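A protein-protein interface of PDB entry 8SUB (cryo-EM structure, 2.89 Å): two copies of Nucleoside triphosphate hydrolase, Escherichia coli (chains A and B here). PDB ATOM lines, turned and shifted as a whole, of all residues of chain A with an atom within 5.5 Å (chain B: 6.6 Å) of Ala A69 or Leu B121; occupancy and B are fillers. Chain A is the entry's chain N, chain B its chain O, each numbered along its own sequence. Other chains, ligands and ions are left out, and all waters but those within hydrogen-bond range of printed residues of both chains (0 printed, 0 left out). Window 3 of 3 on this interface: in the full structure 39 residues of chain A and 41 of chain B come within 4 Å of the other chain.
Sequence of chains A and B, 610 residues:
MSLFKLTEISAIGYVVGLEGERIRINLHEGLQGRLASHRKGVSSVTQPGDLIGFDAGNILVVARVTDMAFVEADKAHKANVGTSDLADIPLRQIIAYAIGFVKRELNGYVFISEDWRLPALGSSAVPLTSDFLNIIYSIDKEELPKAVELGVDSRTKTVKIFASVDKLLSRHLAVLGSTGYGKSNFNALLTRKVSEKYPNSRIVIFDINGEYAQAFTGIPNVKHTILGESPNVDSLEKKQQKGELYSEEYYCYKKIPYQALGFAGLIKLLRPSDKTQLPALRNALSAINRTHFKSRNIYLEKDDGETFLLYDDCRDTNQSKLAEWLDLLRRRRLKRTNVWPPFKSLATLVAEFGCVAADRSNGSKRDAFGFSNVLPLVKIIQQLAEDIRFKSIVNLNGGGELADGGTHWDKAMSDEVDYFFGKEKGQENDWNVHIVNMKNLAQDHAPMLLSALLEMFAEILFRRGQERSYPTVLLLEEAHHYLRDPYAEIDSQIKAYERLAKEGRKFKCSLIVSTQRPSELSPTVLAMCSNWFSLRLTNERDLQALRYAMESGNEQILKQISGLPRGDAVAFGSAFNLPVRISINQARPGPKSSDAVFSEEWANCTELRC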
ATOM      1  N   ASP A  67     -29.052   4.039  23.446  1.00  0.00           N
ATOM      2  CA  ASP A  67     -29.446   2.799  22.782  1.00  0.00           C
ATOM      3  C   ASP A  67     -28.839   2.744  21.388  1.00  0.00           C
ATOM      4  O   ASP A  67     -28.606   3.775  20.760  1.00  0.00           O
ATOM      5  CB  ASP A  67     -30.966   2.678  22.667  1.00  0.00           C
ATOM      6  CG  ASP A  67     -31.619   2.245  23.951  1.00  0.00           C
ATOM      7  OD1 ASP A  67     -31.023   1.433  24.680  1.00  0.00           O
ATOM      8  OD2 ASP A  67     -32.733   2.728  24.241  1.00  0.00           O
ATOM      9  N   MET A  68     -28.593   1.525  20.907  1.00  0.00           N
ATOM     10  CA  MET A  68     -28.099   1.272  19.557  1.00  0.00           C
ATOM     11  C   MET A  68     -28.605  -0.094  19.101  1.00  0.00           C
ATOM     12  O   MET A  68     -28.561  -1.049  19.875  1.00  0.00           O
ATOM     13  CB  MET A  68     -26.565   1.307  19.500  1.00  0.00           C
ATOM     14  CG  MET A  68     -25.931   2.602  19.978  1.00  0.00           C
ATOM     15  SD  MET A  68     -24.172   2.752  19.664  1.00  0.00           S
ATOM     16  CE  MET A  68     -24.158   2.930  17.892  1.00  0.00           C
ATOM     17  N   ALA A  69     -29.074  -0.192  17.857  1.00  0.00           N
ATOM     18  CA  ALA A  69     -29.620  -1.462  17.384  1.00  0.00           C
ATOM     19  C   ALA A  69     -29.751  -1.474  15.867  1.00  0.00           C
ATOM     20  O   ALA A  69     -29.807  -0.429  15.219  1.00  0.00           O
ATOM     21  CB  ALA A  69     -30.978  -1.756  18.019  1.00  0.00           C
ATOM     22  N   PHE A  70     -29.802  -2.689  15.316  1.00  0.00           N
ATOM     23  CA  PHE A  70     -30.185  -2.904  13.924  1.00  0.00           C
ATOM     24  C   PHE A  70     -31.696  -2.794  13.784  1.00  0.00           C
ATOM     25  O   PHE A  70     -32.443  -3.396  14.558  1.00  0.00           O
ATOM     26  CB  PHE A  70     -29.737  -4.286  13.449  1.00  0.00           C
ATOM     27  CG  PHE A  70     -28.314  -4.352  12.976  1.00  0.00           C
ATOM     28  CD1 PHE A  70     -27.843  -3.483  12.019  1.00  0.00           C
ATOM     29  CD2 PHE A  70     -27.449  -5.289  13.491  1.00  0.00           C
ATOM     30  CE1 PHE A  70     -26.542  -3.550  11.596  1.00  0.00           C
ATOM     31  CE2 PHE A  70     -26.151  -5.355  13.069  1.00  0.00           C
ATOM     32  CZ  PHE A  70     -25.698  -4.487  12.125  1.00  0.00           C
ATOM     33  N   VAL A  71     -32.155  -2.044  12.791  1.00  0.00           N
ATOM     34  CA  VAL A  71     -33.588  -1.884  12.586  1.00  0.00           C
ATOM     35  C   VAL A  71     -34.158  -3.131  11.941  1.00  0.00           C
ATOM     36  O   VAL A  71     -34.012  -3.333  10.738  1.00  0.00           O
ATOM     37  CB  VAL A  71     -33.906  -0.650  11.733  1.00  0.00           C
ATOM     38  CG1 VAL A  71     -35.400  -0.541  11.505  1.00  0.00           C
ATOM     39  CG2 VAL A  71     -33.385   0.597  12.399  1.00  0.00           C
ATOM     40  N   LEU A  91     -30.045  -1.194   8.414  1.00  0.00           N
ATOM     41  CA  LEU A  91     -30.076   0.180   8.887  1.00  0.00           C
ATOM     42  C   LEU A  91     -29.888   0.198  10.398  1.00  0.00           C
ATOM     43  O   LEU A  91     -30.318  -0.725  11.093  1.00  0.00           O
ATOM     44  CB  LEU A  91     -31.404   0.834   8.490  1.00  0.00           C
ATOM     45  CG  LEU A  91     -31.823   2.219   8.977  1.00  0.00           C
ATOM     46  CD1 LEU A  91     -31.123   3.307   8.192  1.00  0.00           C
ATOM     47  CD2 LEU A  91     -33.324   2.360   8.860  1.00  0.00           C
ATOM     48  N   ARG A  92     -29.231   1.242  10.904  1.00  0.00           N
ATOM     49  CA  ARG A  92     -28.923   1.369  12.321  1.00  0.00           C
ATOM     50  C   ARG A  92     -29.486   2.670  12.882  1.00  0.00           C
ATOM     51  O   ARG A  92     -29.550   3.684  12.186  1.00  0.00           O
ATOM     52  CB  ARG A  92     -27.414   1.312  12.560  1.00  0.00           C
ATOM     53  CG  ARG A  92     -26.715   0.156  11.875  1.00  0.00           C
ATOM     54  CD  ARG A  92     -25.208   0.301  11.928  1.00  0.00           C
ATOM     55  NE  ARG A  92     -24.717   1.310  11.001  1.00  0.00           N
ATOM     56  CZ  ARG A  92     -23.449   1.683  10.902  1.00  0.00           C
ATOM     57  NH1 ARG A  92     -22.511   1.142  11.657  1.00  0.00           N
ATOM     58  NH2 ARG A  92     -23.116   2.621  10.021  1.00  0.00           N
ATOM     59  N   GLN A  93     -29.871   2.640  14.161  1.00  0.00           N
ATOM     60  CA  GLN A  93     -30.537   3.755  14.823  1.00  0.00           C
ATOM     61  C   GLN A  93     -29.934   4.014  16.202  1.00  0.00           C
ATOM     62  O   GLN A  93     -29.191   3.197  16.742  1.00  0.00           O
ATOM     63  CB  GLN A  93     -32.037   3.491  14.954  1.00  0.00           C
ATOM     64  CG  GLN A  93     -32.842   3.926  13.764  1.00  0.00           C
ATOM     65  CD  GLN A  93     -34.321   3.915  14.044  1.00  0.00           C
ATOM     66  OE1 GLN A  93     -34.752   3.554  15.137  1.00  0.00           O
ATOM     67  NE2 GLN A  93     -35.112   4.306  13.057  1.00  0.00           N
ATOM     68  N   VAL B  15     -22.990  -9.409  17.136  1.00  0.00           N
ATOM     69  CA  VAL B  15     -23.710  -8.478  18.000  1.00  0.00           C
ATOM     70  C   VAL B  15     -24.766  -7.729  17.200  1.00  0.00           C
ATOM     71  O   VAL B  15     -24.507  -7.261  16.090  1.00  0.00           O
ATOM     72  CB  VAL B  15     -22.725  -7.502  18.668  1.00  0.00           C
ATOM     73  CG1 VAL B  15     -23.455  -6.505  19.538  1.00  0.00           C
ATOM     74  CG2 VAL B  15     -21.697  -8.259  19.478  1.00  0.00           C
ATOM     75  N   VAL B  16     -25.966  -7.595  17.772  1.00  0.00           N
ATOM     76  CA  VAL B  16     -27.097  -7.001  17.071  1.00  0.00           C
ATOM     77  C   VAL B  16     -27.822  -5.946  17.901  1.00  0.00           C
ATOM     78  O   VAL B  16     -28.797  -5.366  17.427  1.00  0.00           O
ATOM     79  CB  VAL B  16     -28.078  -8.104  16.599  1.00  0.00           C
ATOM     80  CG1 VAL B  16     -28.752  -8.791  17.772  1.00  0.00           C
ATOM     81  CG2 VAL B  16     -29.073  -7.608  15.559  1.00  0.00           C
ATOM     82  N   GLY B  17     -27.374  -5.658  19.121  1.00  0.00           N
ATOM     83  CA  GLY B  17     -27.992  -4.608  19.915  1.00  0.00           C
ATOM     84  C   GLY B  17     -27.316  -4.311  21.240  1.00  0.00           C
ATOM     85  O   GLY B  17     -26.794  -5.218  21.888  1.00  0.00           O
ATOM     86  N   LEU B  18     -27.318  -3.044  21.655  1.00  0.00           N
ATOM     87  CA  LEU B  18     -26.757  -2.619  22.939  1.00  0.00           C
ATOM     88  C   LEU B  18     -27.769  -1.709  23.618  1.00  0.00           C
ATOM     89  O   LEU B  18     -27.954  -0.570  23.188  1.00  0.00           O
ATOM     90  CB  LEU B  18     -25.430  -1.886  22.753  1.00  0.00           C
ATOM     91  CG  LEU B  18     -24.274  -2.554  22.019  1.00  0.00           C
ATOM     92  CD1 LEU B  18     -23.368  -1.494  21.449  1.00  0.00           C
ATOM     93  CD2 LEU B  18     -23.510  -3.476  22.934  1.00  0.00           C
ATOM     94  N   GLU B  19     -28.413  -2.188  24.679  1.00  0.00           N
ATOM     95  CA  GLU B  19     -29.516  -1.475  25.328  1.00  0.00           C
ATOM     96  C   GLU B  19     -29.162  -1.219  26.788  1.00  0.00           C
ATOM     97  O   GLU B  19     -29.539  -1.995  27.667  1.00  0.00           O
ATOM     98  CB  GLU B  19     -30.812  -2.269  25.228  1.00  0.00           C
ATOM     99  CG  GLU B  19     -31.421  -2.316  23.841  1.00  0.00           C
ATOM    100  CD  GLU B  19     -31.098  -3.605  23.114  1.00  0.00           C
ATOM    101  OE1 GLU B  19     -30.555  -4.525  23.762  1.00  0.00           O
ATOM    102  OE2 GLU B  19     -31.377  -3.695  21.900  1.00  0.00           O
ATOM    103  N   PRO B 119     -18.587  -3.977  23.073  1.00  0.00           N
ATOM    104  CA  PRO B 119     -18.253  -4.216  21.667  1.00  0.00           C
ATOM    105  C   PRO B 119     -19.143  -3.399  20.736  1.00  0.00           C
ATOM    106  O   PRO B 119     -20.126  -2.789  21.146  1.00  0.00           O
ATOM    107  CB  PRO B 119     -18.502  -5.713  21.504  1.00  0.00           C
ATOM    108  CG  PRO B 119     -19.523  -6.028  22.498  1.00  0.00           C
ATOM    109  CD  PRO B 119     -19.279  -5.131  23.670  1.00  0.00           C
ATOM    110  N   ALA B 120     -18.779  -3.398  19.460  1.00  0.00           N
ATOM    111  CA  ALA B 120     -19.504  -2.639  18.451  1.00  0.00           C
ATOM    112  C   ALA B 120     -20.467  -3.535  17.681  1.00  0.00           C
ATOM    113  O   ALA B 120     -20.282  -4.749  17.591  1.00  0.00           O
ATOM    114  CB  ALA B 120     -18.527  -1.975  17.488  1.00  0.00           C
ATOM    115  N   LEU B 121     -21.506  -2.917  17.117  1.00  0.00           N
ATOM    116  CA  LEU B 121     -22.480  -3.661  16.328  1.00  0.00           C
ATOM    117  C   LEU B 121     -21.817  -4.334  15.135  1.00  0.00           C
ATOM    118  O   LEU B 121     -21.025  -3.725  14.415  1.00  0.00           O
ATOM    119  CB  LEU B 121     -23.605  -2.747  15.847  1.00  0.00           C
ATOM    120  CG  LEU B 121     -24.834  -2.517  16.725  1.00  0.00           C
ATOM    121  CD1 LEU B 121     -24.477  -1.757  17.958  1.00  0.00           C
ATOM    122  CD2 LEU B 121     -25.879  -1.762  15.938  1.00  0.00           C
ATOM    123  N   GLY B 122     -22.149  -5.603  14.932  1.00  0.00           N
ATOM    124  CA  GLY B 122     -21.590  -6.385  13.860  1.00  0.00           C
ATOM    125  C   GLY B 122     -20.367  -7.195  14.217  1.00  0.00           C
ATOM    126  O   GLY B 122     -19.977  -8.064  13.432  1.00  0.00           O
ATOM    127  N   SER B 123     -19.754  -6.951  15.372  1.00  0.00           N
ATOM    128  CA  SER B 123     -18.567  -7.698  15.758  1.00  0.00           C
ATOM    129  C   SER B 123     -18.936  -9.138  16.096  1.00  0.00           C
ATOM    130  O   SER B 123     -20.092  -9.461  16.364  1.00  0.00           O
ATOM    131  CB  SER B 123     -17.873  -7.030  16.939  1.00  0.00           C
ATOM    132  OG  SER B 123     -18.706  -7.028  18.076  1.00  0.00           O
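No position is printed for both chains. Of the 8 pairs that touch across the chains among the printed residues, none has its exchanged pair printed and touching as well.
The backbone carbonyl oxygen (O) of Met A68 lies within hydrogen-bond range of the backbone NH (N) of Leu B18, at 2.9 Å.
Of the printed residues of chain B, Ala A69 touches Val B16 and Leu B121. Printed residues of chain A within 4 Å of Leu B121: Ala A69 (3.9 Å). Printed residues of chain A within 4 Å of Glu B19: Asp A67 (3.3 Å). Printed residues of chain A within 4 Å of Leu B18: Asp A67 and Met A68. Of the printed residues of chain B, Asp A67 touches Leu B18 and Glu B19. Printed residues of chain A within 4 Å of Val B16: Ala A69 and Phe A70. Printed residues of chain A within 4 Å of Val B15: Phe A70 (3.9 Å). Arg A92 touches none of the printed residues of chain B. The nearest printed residue of chain A that does not touch Leu B121 is Met A68 (4.02 Å). The nearest printed residue of chain A that does not touch Leu B18 is Ala A69 (5.1 Å).
Among the printed residues, merely in contact across the chains: Asp A67 with Glu B19 (3.3 Å), Phe A70 with Val B16 (3.5 Å), Met A68 with Gly B17 (3.6 Å), Asp A67 with Leu B18 (3.7 Å), Ala A69 with Leu B121 (3.9 Å), Phe A70 with Val B15 (3.9 Å) and Ala A69 with Val B16 (3.99 Å).
Along chain A the printed residues that touch a printed residue of chain B span positions 67 to 70. Of the 10 printed residues of chain B, 6 touch a printed residue of chain A. Hydrophobic or aromatic side chains of chain B within 4 Å of the printed part of chain A: Val B16 and Leu B121. Among the printed residues, 8 pairs touch across the chains. Among the printed residues, no Asp or Glu carboxylate lies within 4 Å of a Lys or Arg side-chain nitrogen of the other chain.
N of Gln A93 lies within hydrogen-bond range of O of Ala A69 (3.2 Å). The backbone carbonyl oxygen of Val B15 lies within hydrogen-bond range of the backbone NH of Gly B122, 3.1 Å away. N of Val B15 sits at hydrogen-bond distance from O of Ser B123, 3.0 Å away.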
